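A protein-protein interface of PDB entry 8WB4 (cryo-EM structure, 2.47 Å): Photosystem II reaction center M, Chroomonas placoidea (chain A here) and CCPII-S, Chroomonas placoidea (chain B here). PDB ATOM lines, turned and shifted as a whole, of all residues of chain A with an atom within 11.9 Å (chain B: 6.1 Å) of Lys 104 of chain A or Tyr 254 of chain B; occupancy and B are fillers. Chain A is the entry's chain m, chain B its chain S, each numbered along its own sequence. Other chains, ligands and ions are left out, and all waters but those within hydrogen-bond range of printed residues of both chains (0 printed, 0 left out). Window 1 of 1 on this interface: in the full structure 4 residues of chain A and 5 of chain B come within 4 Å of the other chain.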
ATOM      1  N   LEU A  94      34.966  -9.255  14.237  1.00  0.00           N
ATOM      2  CA  LEU A  94      34.459  -8.031  14.847  1.00  0.00           C
ATOM      3  C   LEU A  94      32.988  -8.163  15.203  1.00  0.00           C
ATOM      4  O   LEU A  94      32.559  -7.724  16.278  1.00  0.00           O
ATOM      5  CB  LEU A  94      34.674  -6.845  13.912  1.00  0.00           C
ATOM      6  CG  LEU A  94      35.894  -5.975  14.196  1.00  0.00           C
ATOM      7  CD1 LEU A  94      35.810  -5.413  15.601  1.00  0.00           C
ATOM      8  CD2 LEU A  94      37.170  -6.766  14.012  1.00  0.00           C
ATOM      9  N   THR A  95      32.199  -8.764  14.312  1.00  0.00           N
ATOM     10  CA  THR A  95      30.787  -8.971  14.600  1.00  0.00           C
ATOM     11  C   THR A  95      30.605  -9.890  15.797  1.00  0.00           C
ATOM     12  O   THR A  95      29.776  -9.617  16.672  1.00  0.00           O
ATOM     13  CB  THR A  95      30.083  -9.538  13.371  1.00  0.00           C
ATOM     14  OG1 THR A  95      30.369  -8.712  12.238  1.00  0.00           O
ATOM     15  CG2 THR A  95      28.587  -9.574  13.590  1.00  0.00           C
ATOM     16  N   LEU A  96      31.383 -10.974  15.864  1.00  0.00           N
ATOM     17  CA  LEU A  96      31.294 -11.866  17.015  1.00  0.00           C
ATOM     18  C   LEU A  96      31.625 -11.137  18.306  1.00  0.00           C
ATOM     19  O   LEU A  96      30.917 -11.284  19.310  1.00  0.00           O
ATOM     20  CB  LEU A  96      32.233 -13.053  16.834  1.00  0.00           C
ATOM     21  CG  LEU A  96      31.726 -14.289  16.106  1.00  0.00           C
ATOM     22  CD1 LEU A  96      32.776 -15.363  16.209  1.00  0.00           C
ATOM     23  CD2 LEU A  96      30.432 -14.759  16.717  1.00  0.00           C
ATOM     24  N   TYR A  97      32.701 -10.351  18.305  1.00  0.00           N
ATOM     25  CA  TYR A  97      33.103  -9.671  19.530  1.00  0.00           C
ATOM     26  C   TYR A  97      32.066  -8.649  19.967  1.00  0.00           C
ATOM     27  O   TYR A  97      31.741  -8.562  21.155  1.00  0.00           O
ATOM     28  CB  TYR A  97      34.464  -9.006  19.348  1.00  0.00           C
ATOM     29  CG  TYR A  97      34.862  -8.152  20.524  1.00  0.00           C
ATOM     30  CD1 TYR A  97      35.279  -8.728  21.713  1.00  0.00           C
ATOM     31  CD2 TYR A  97      34.815  -6.769  20.449  1.00  0.00           C
ATOM     32  CE1 TYR A  97      35.639  -7.953  22.789  1.00  0.00           C
ATOM     33  CE2 TYR A  97      35.173  -5.988  21.519  1.00  0.00           C
ATOM     34  CZ  TYR A  97      35.586  -6.584  22.686  1.00  0.00           C
ATOM     35  OH  TYR A  97      35.946  -5.805  23.758  1.00  0.00           O
ATOM     36  N   ILE A  98      31.535  -7.865  19.028  1.00  0.00           N
ATOM     37  CA  ILE A  98      30.546  -6.855  19.393  1.00  0.00           C
ATOM     38  C   ILE A  98      29.267  -7.513  19.891  1.00  0.00           C
ATOM     39  O   ILE A  98      28.659  -7.060  20.868  1.00  0.00           O
ATOM     40  CB  ILE A  98      30.288  -5.915  18.204  1.00  0.00           C
ATOM     41  CG1 ILE A  98      31.529  -5.066  17.936  1.00  0.00           C
ATOM     42  CG2 ILE A  98      29.092  -5.030  18.474  1.00  0.00           C
ATOM     43  CD1 ILE A  98      31.427  -4.210  16.710  1.00  0.00           C
ATOM     44  N   GLN A  99      28.846  -8.598  19.239  1.00  0.00           N
ATOM     45  CA  GLN A  99      27.671  -9.331  19.690  1.00  0.00           C
ATOM     46  C   GLN A  99      27.862  -9.865  21.105  1.00  0.00           C
ATOM     47  O   GLN A  99      26.973  -9.730  21.955  1.00  0.00           O
ATOM     48  CB  GLN A  99      27.387 -10.466  18.709  1.00  0.00           C
ATOM     49  CG  GLN A  99      26.454 -11.528  19.215  1.00  0.00           C
ATOM     50  CD  GLN A  99      27.171 -12.755  19.718  1.00  0.00           C
ATOM     51  OE1 GLN A  99      28.371 -12.914  19.514  1.00  0.00           O
ATOM     52  NE2 GLN A  99      26.435 -13.636  20.382  1.00  0.00           N
ATOM     53  N   SER A 100      29.024 -10.459  21.379  1.00  0.00           N
ATOM     54  CA  SER A 100      29.289 -10.995  22.709  1.00  0.00           C
ATOM     55  C   SER A 100      29.334  -9.889  23.754  1.00  0.00           C
ATOM     56  O   SER A 100      28.811 -10.052  24.863  1.00  0.00           O
ATOM     57  CB  SER A 100      30.598 -11.780  22.699  1.00  0.00           C
ATOM     58  OG  SER A 100      30.884 -12.302  23.981  1.00  0.00           O
ATOM     59  N   GLU A 101      29.952  -8.757  23.420  1.00  0.00           N
ATOM     60  CA  GLU A 101      30.044  -7.661  24.376  1.00  0.00           C
ATOM     61  C   GLU A 101      28.675  -7.073  24.679  1.00  0.00           C
ATOM     62  O   GLU A 101      28.387  -6.728  25.827  1.00  0.00           O
ATOM     63  CB  GLU A 101      30.990  -6.586  23.854  1.00  0.00           C
ATOM     64  CG  GLU A 101      32.438  -7.006  23.886  1.00  0.00           C
ATOM     65  CD  GLU A 101      32.893  -7.408  25.272  1.00  0.00           C
ATOM     66  OE1 GLU A 101      32.523  -6.720  26.245  1.00  0.00           O
ATOM     67  OE2 GLU A 101      33.616  -8.418  25.392  1.00  0.00           O
ATOM     68  N   SER A 102      27.813  -6.957  23.671  1.00  0.00           N
ATOM     69  CA  SER A 102      26.471  -6.452  23.929  1.00  0.00           C
ATOM     70  C   SER A 102      25.621  -7.443  24.707  1.00  0.00           C
ATOM     71  O   SER A 102      24.806  -7.031  25.539  1.00  0.00           O
ATOM     72  CB  SER A 102      25.788  -6.078  22.621  1.00  0.00           C
ATOM     73  OG  SER A 102      26.280  -4.831  22.177  1.00  0.00           O
ATOM     74  N   ARG A 103      25.791  -8.742  24.465  1.00  0.00           N
ATOM     75  CA  ARG A 103      25.093  -9.716  25.296  1.00  0.00           C
ATOM     76  C   ARG A 103      25.560  -9.638  26.744  1.00  0.00           C
ATOM     77  O   ARG A 103      24.744  -9.717  27.669  1.00  0.00           O
ATOM     78  CB  ARG A 103      25.278 -11.123  24.737  1.00  0.00           C
ATOM     79  CG  ARG A 103      24.524 -12.165  25.524  1.00  0.00           C
ATOM     80  CD  ARG A 103      24.306 -13.431  24.734  1.00  0.00           C
ATOM     81  NE  ARG A 103      23.536 -14.399  25.505  1.00  0.00           N
ATOM     82  CZ  ARG A 103      22.243 -14.628  25.335  1.00  0.00           C
ATOM     83  NH1 ARG A 103      21.547 -14.000  24.405  1.00  0.00           N
ATOM     84  NH2 ARG A 103      21.633 -15.514  26.115  1.00  0.00           N
ATOM     85  N   LYS A 104      26.867  -9.474  26.965  1.00  0.00           N
ATOM     86  CA  LYS A 104      27.355  -9.281  28.328  1.00  0.00           C
ATOM     87  C   LYS A 104      26.811  -7.999  28.943  1.00  0.00           C
ATOM     88  O   LYS A 104      26.482  -7.975  30.133  1.00  0.00           O
ATOM     89  CB  LYS A 104      28.883  -9.267  28.358  1.00  0.00           C
ATOM     90  CG  LYS A 104      29.516 -10.642  28.408  1.00  0.00           C
ATOM     91  CD  LYS A 104      30.990 -10.567  28.758  1.00  0.00           C
ATOM     92  CE  LYS A 104      31.760  -9.764  27.732  1.00  0.00           C
ATOM     93  NZ  LYS A 104      33.216  -9.753  28.027  1.00  0.00           N
ATOM     94  N   ALA A 105      26.724  -6.927  28.157  1.00  0.00           N
ATOM     95  CA  ALA A 105      26.229  -5.655  28.667  1.00  0.00           C
ATOM     96  C   ALA A 105      24.755  -5.716  29.032  1.00  0.00           C
ATOM     97  O   ALA A 105      24.336  -5.069  29.997  1.00  0.00           O
ATOM     98  CB  ALA A 105      26.468  -4.549  27.641  1.00  0.00           C
ATOM     99  N   ALA A 106      23.954  -6.459  28.276  1.00  0.00           N
ATOM    100  CA  ALA A 106      22.555  -6.642  28.628  1.00  0.00           C
ATOM    101  C   ALA A 106      22.341  -7.713  29.687  1.00  0.00           C
ATOM    102  O   ALA A 106      21.256  -7.773  30.273  1.00  0.00           O
ATOM    103  CB  ALA A 106      21.735  -6.989  27.389  1.00  0.00           C
ATOM    104  N   GLU A 107      23.337  -8.563  29.938  1.00  0.00           N
ATOM    105  CA  GLU A 107      23.234  -9.496  31.053  1.00  0.00           C
ATOM    106  C   GLU A 107      23.251  -8.763  32.387  1.00  0.00           C
ATOM    107  O   GLU A 107      22.643  -9.229  33.357  1.00  0.00           O
ATOM    108  CB  GLU A 107      24.366 -10.520  30.994  1.00  0.00           C
ATOM    109  N   THR A 108      23.935  -7.626  32.453  1.00  0.00           N
ATOM    110  CA  THR A 108      23.992  -6.830  33.669  1.00  0.00           C
ATOM    111  C   THR A 108      22.672  -6.109  33.897  1.00  0.00           C
ATOM    112  O   THR A 108      22.017  -5.687  32.946  1.00  0.00           O
ATOM    113  CB  THR A 108      25.126  -5.798  33.614  1.00  0.00           C
ATOM    114  OG1 THR A 108      24.814  -4.801  32.634  1.00  0.00           O
ATOM    115  CG2 THR A 108      26.434  -6.471  33.241  1.00  0.00           C
ATOM    116  N   PRO B 245      34.436  -7.072  35.997  1.00  0.00           N
ATOM    117  CA  PRO B 245      33.693  -8.151  36.663  1.00  0.00           C
ATOM    118  C   PRO B 245      33.463  -9.381  35.800  1.00  0.00           C
ATOM    119  O   PRO B 245      33.091 -10.427  36.343  1.00  0.00           O
ATOM    120  CB  PRO B 245      32.365  -7.481  37.029  1.00  0.00           C
ATOM    121  CG  PRO B 245      32.199  -6.421  36.000  1.00  0.00           C
ATOM    122  CD  PRO B 245      33.579  -5.914  35.694  1.00  0.00           C
ATOM    123  N   SER B 246      33.664  -9.298  34.490  1.00  0.00           N
ATOM    124  CA  SER B 246      33.396 -10.407  33.583  1.00  0.00           C
ATOM    125  C   SER B 246      34.662 -10.846  32.861  1.00  0.00           C
ATOM    126  O   SER B 246      34.644 -11.132  31.663  1.00  0.00           O
ATOM    127  CB  SER B 246      32.317 -10.032  32.573  1.00  0.00           C
ATOM    128  OG  SER B 246      32.759  -8.984  31.731  1.00  0.00           O
ATOM    129  N   LYS B 249      35.151 -15.124  33.209  1.00  0.00           N
ATOM    130  CA  LYS B 249      33.861 -15.794  33.186  1.00  0.00           C
ATOM    131  C   LYS B 249      33.344 -15.869  31.757  1.00  0.00           C
ATOM    132  O   LYS B 249      33.521 -14.933  30.973  1.00  0.00           O
ATOM    133  CB  LYS B 249      32.849 -15.061  34.066  1.00  0.00           C
ATOM    134  CG  LYS B 249      33.360 -14.749  35.457  1.00  0.00           C
ATOM    135  CD  LYS B 249      32.309 -14.040  36.285  1.00  0.00           C
ATOM    136  CE  LYS B 249      32.865 -13.615  37.629  1.00  0.00           C
ATOM    137  NZ  LYS B 249      33.987 -12.653  37.475  1.00  0.00           N
ATOM    138  N   SER B 250      32.709 -16.988  31.422  1.00  0.00           N
ATOM    139  CA  SER B 250      32.137 -17.157  30.098  1.00  0.00           C
ATOM    140  C   SER B 250      30.827 -16.382  29.994  1.00  0.00           C
ATOM    141  O   SER B 250      30.344 -15.787  30.960  1.00  0.00           O
ATOM    142  CB  SER B 250      31.925 -18.637  29.792  1.00  0.00           C
ATOM    143  OG  SER B 250      30.924 -19.192  30.624  1.00  0.00           O
ATOM    144  N   LEU B 251      30.244 -16.387  28.797  1.00  0.00           N
ATOM    145  CA  LEU B 251      28.996 -15.667  28.578  1.00  0.00           C
ATOM    146  C   LEU B 251      27.863 -16.259  29.408  1.00  0.00           C
ATOM    147  O   LEU B 251      27.141 -15.528  30.096  1.00  0.00           O
ATOM    148  CB  LEU B 251      28.654 -15.683  27.091  1.00  0.00           C
ATOM    149  CG  LEU B 251      27.536 -14.785  26.575  1.00  0.00           C
ATOM    150  CD1 LEU B 251      27.669 -13.400  27.157  1.00  0.00           C
ATOM    151  CD2 LEU B 251      27.611 -14.728  25.067  1.00  0.00           C
ATOM    152  N   ILE B 252      27.703 -17.583  29.372  1.00  0.00           N
ATOM    153  CA  ILE B 252      26.683 -18.237  30.184  1.00  0.00           C
ATOM    154  C   ILE B 252      26.988 -18.069  31.666  1.00  0.00           C
ATOM    155  O   ILE B 252      26.085 -17.829  32.476  1.00  0.00           O
ATOM    156  CB  ILE B 252      26.563 -19.720  29.793  1.00  0.00           C
ATOM    157  CG1 ILE B 252      26.035 -19.853  28.366  1.00  0.00           C
ATOM    158  CG2 ILE B 252      25.660 -20.462  30.763  1.00  0.00           C
ATOM    159  CD1 ILE B 252      25.999 -21.276  27.861  1.00  0.00           C
ATOM    160  N   GLU B 253      28.260 -18.196  32.047  1.00  0.00           N
ATOM    161  CA  GLU B 253      28.629 -18.072  33.453  1.00  0.00           C
ATOM    162  C   GLU B 253      28.351 -16.671  33.981  1.00  0.00           C
ATOM    163  O   GLU B 253      27.829 -16.512  35.089  1.00  0.00           O
ATOM    164  CB  GLU B 253      30.100 -18.434  33.637  1.00  0.00           C
ATOM    165  CG  GLU B 253      30.570 -18.410  35.075  1.00  0.00           C
ATOM    166  CD  GLU B 253      32.010 -18.847  35.218  1.00  0.00           C
ATOM    167  OE1 GLU B 253      32.670 -19.070  34.181  1.00  0.00           O
ATOM    168  OE2 GLU B 253      32.482 -18.970  36.366  1.00  0.00           O
ATOM    169  N   TYR B 254      28.692 -15.642  33.204  1.00  0.00           N
ATOM    170  CA  TYR B 254      28.427 -14.272  33.622  1.00  0.00           C
ATOM    171  C   TYR B 254      26.954 -13.911  33.525  1.00  0.00           C
ATOM    172  O   TYR B 254      26.512 -12.976  34.200  1.00  0.00           O
ATOM    173  CB  TYR B 254      29.266 -13.300  32.789  1.00  0.00           C
ATOM    174  CG  TYR B 254      29.231 -11.872  33.276  1.00  0.00           C
ATOM    175  CD1 TYR B 254      29.701 -11.538  34.536  1.00  0.00           C
ATOM    176  CD2 TYR B 254      28.745 -10.855  32.469  1.00  0.00           C
ATOM    177  CE1 TYR B 254      29.677 -10.236  34.984  1.00  0.00           C
ATOM    178  CE2 TYR B 254      28.718  -9.548  32.906  1.00  0.00           C
ATOM    179  CZ  TYR B 254      29.185  -9.245  34.165  1.00  0.00           C
ATOM    180  OH  TYR B 254      29.162  -7.945  34.609  1.00  0.00           O
ATOM    181  N   SER B 255      26.187 -14.617  32.693  1.00  0.00           N
ATOM    182  CA  SER B 255      24.744 -14.432  32.663  1.00  0.00           C
ATOM    183  C   SER B 255      24.042 -15.110  33.831  1.00  0.00           C
ATOM    184  O   SER B 255      22.977 -14.644  34.249  1.00  0.00           O
ATOM    185  CB  SER B 255      24.175 -14.955  31.345  1.00  0.00           C
ATOM    186  OG  SER B 255      24.727 -14.254  30.246  1.00  0.00           O
ATOM    187  N   GLU B 256      24.600 -16.204  34.352  1.00  0.00           N
ATOM    188  CA  GLU B 256      24.020 -16.837  35.531  1.00  0.00           C
ATOM    189  C   GLU B 256      24.129 -15.931  36.748  1.00  0.00           C
ATOM    190  O   GLU B 256      23.204 -15.867  37.565  1.00  0.00           O
ATOM    191  CB  GLU B 256      24.691 -18.183  35.795  1.00  0.00           C
ATOM    192  CG  GLU B 256      24.358 -19.241  34.761  1.00  0.00           C
ATOM    193  CD  GLU B 256      22.865 -19.463  34.618  1.00  0.00           C
ATOM    194  OE1 GLU B 256      22.163 -19.487  35.651  1.00  0.00           O
ATOM    195  OE2 GLU B 256      22.392 -19.606  33.471  1.00  0.00           O
ATOM    196  N   GLU B 257      25.252 -15.235  36.895  1.00  0.00           N
ATOM    197  CA  GLU B 257      25.332 -14.167  37.874  1.00  0.00           C
ATOM    198  C   GLU B 257      24.772 -12.888  37.260  1.00  0.00           C
ATOM    199  O   GLU B 257      24.359 -12.858  36.098  1.00  0.00           O
ATOM    200  CB  GLU B 257      26.768 -13.991  38.361  1.00  0.00           C
ATOM    201  CG  GLU B 257      27.722 -13.431  37.330  1.00  0.00           C
ATOM    202  CD  GLU B 257      29.141 -13.343  37.851  1.00  0.00           C
ATOM    203  OE1 GLU B 257      29.613 -14.328  38.457  1.00  0.00           O
ATOM    204  OE2 GLU B 257      29.783 -12.289  37.664  1.00  0.00           O
ATOM    205  N   THR B 258      24.739 -11.818  38.054  1.00  0.00           N
ATOM    206  CA  THR B 258      24.076 -10.563  37.696  1.00  0.00           C
ATOM    207  C   THR B 258      22.586 -10.758  37.431  1.00  0.00           C
ATOM    208  O   THR B 258      21.919  -9.855  36.917  1.00  0.00           O
ATOM    209  CB  THR B 258      24.740  -9.882  36.492  1.00  0.00           C
ATOM    210  OG1 THR B 258      24.472 -10.633  35.302  1.00  0.00           O
ATOM    211  CG2 THR B 258      26.243  -9.786  36.695  1.00  0.00           C
ATOM    212  N   LYS B 259      22.057 -11.934  37.766  1.00  0.00           N
ATOM    213  CA  LYS B 259      20.621 -12.189  37.729  1.00  0.00           C
ATOM    214  C   LYS B 259      20.089 -12.869  38.978  1.00  0.00           C
ATOM    215  O   LYS B 259      18.888 -12.762  39.246  1.00  0.00           O
ATOM    216  CB  LYS B 259      20.252 -13.041  36.509  1.00  0.00           C
ATOM    217  CG  LYS B 259      20.378 -12.309  35.185  1.00  0.00           C
ATOM    218  CD  LYS B 259      19.787 -13.122  34.047  1.00  0.00           C
ATOM    219  CE  LYS B 259      19.831 -12.348  32.740  1.00  0.00           C
ATOM    220  NZ  LYS B 259      19.186 -13.099  31.628  1.00  0.00           N
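Leu 96 of chain A touches none of the printed residues of chain B. Of the printed residues of chain B, Arg 103 of chain A touches Leu 251. Of chain B, only Ser 246, Leu 251 and Tyr 254 come within 4 Å of Lys 104 of chain A. Printed residues of chain B within 4 Å of Thr 108 of chain A: Tyr 254. Ser 246 of chain B touches just one residue of chain A: Lys 104 (3.8 Å). Leu 251 of chain B touches just these residues of chain A: Arg 103 (3.6 Å) and Lys 104 (3.5 Å). No residue of chain A comes within 4 Å of Glu 253 of chain B. Ser 255 of chain B touches one residue of chain A. No residue of chain A comes within 4 Å of Glu 256 of chain B. No residue of chain A comes within 4 Å of Glu 257 of chain B. Lys 259 of chain B touches none of the printed residues of chain A. The nearest residue of chain B that does not touch Lys 104 of chain A is Lys 249 of chain B (5.5 Å).
CD2 of Leu 251 of chain B touches CD of Arg 103 of chain A, 3.6 Å away. Lys 104 of chain A touches Ser 246 of chain B (CD to OG, 3.8 Å). CD1 of Leu 251 of chain B touches CG of Lys 104 of chain A (3.5 Å). Tyr 254 of chain B touches Lys 104 of chain A (CE2 to O, 3.9 Å). CB of Glu 107 of chain A touches OG of Ser 255 of chain B (3.8 Å). Tyr 254 of chain B touches Thr 108 of chain A.
O of Glu 107 of chain A sits at hydrogen-bond distance from OG1 of Thr 258 of chain B (3.0 Å).
Hydrophobic or aromatic side chains of chain B within 4 Å of the printed part of chain A: Leu 251 and Tyr 254. Among the printed residues, no Asp or Glu carboxylate lies within 4 Å of a Lys or Arg side-chain nitrogen of the other chain.
The side-chain hydroxyl (OG1) of Thr 258 of chain B sits at hydrogen-bond distance from the backbone carbonyl oxygen (O) of Tyr 254 of chain B (3.3 Å). The side-chain carboxylate of Glu 101 of chain A is in salt-bridge range of the side-chain amino group of Lys 104 of chain A. The backbone carbonyl oxygen of Ala 105 of chain A is in hydrogen-bond range of the side-chain hydroxyl of Thr 108 of chain A (2.7 Å). O of Leu 251 of chain B sits at hydrogen-bond distance from OG of Ser 255 of chain B (2.7 Å).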
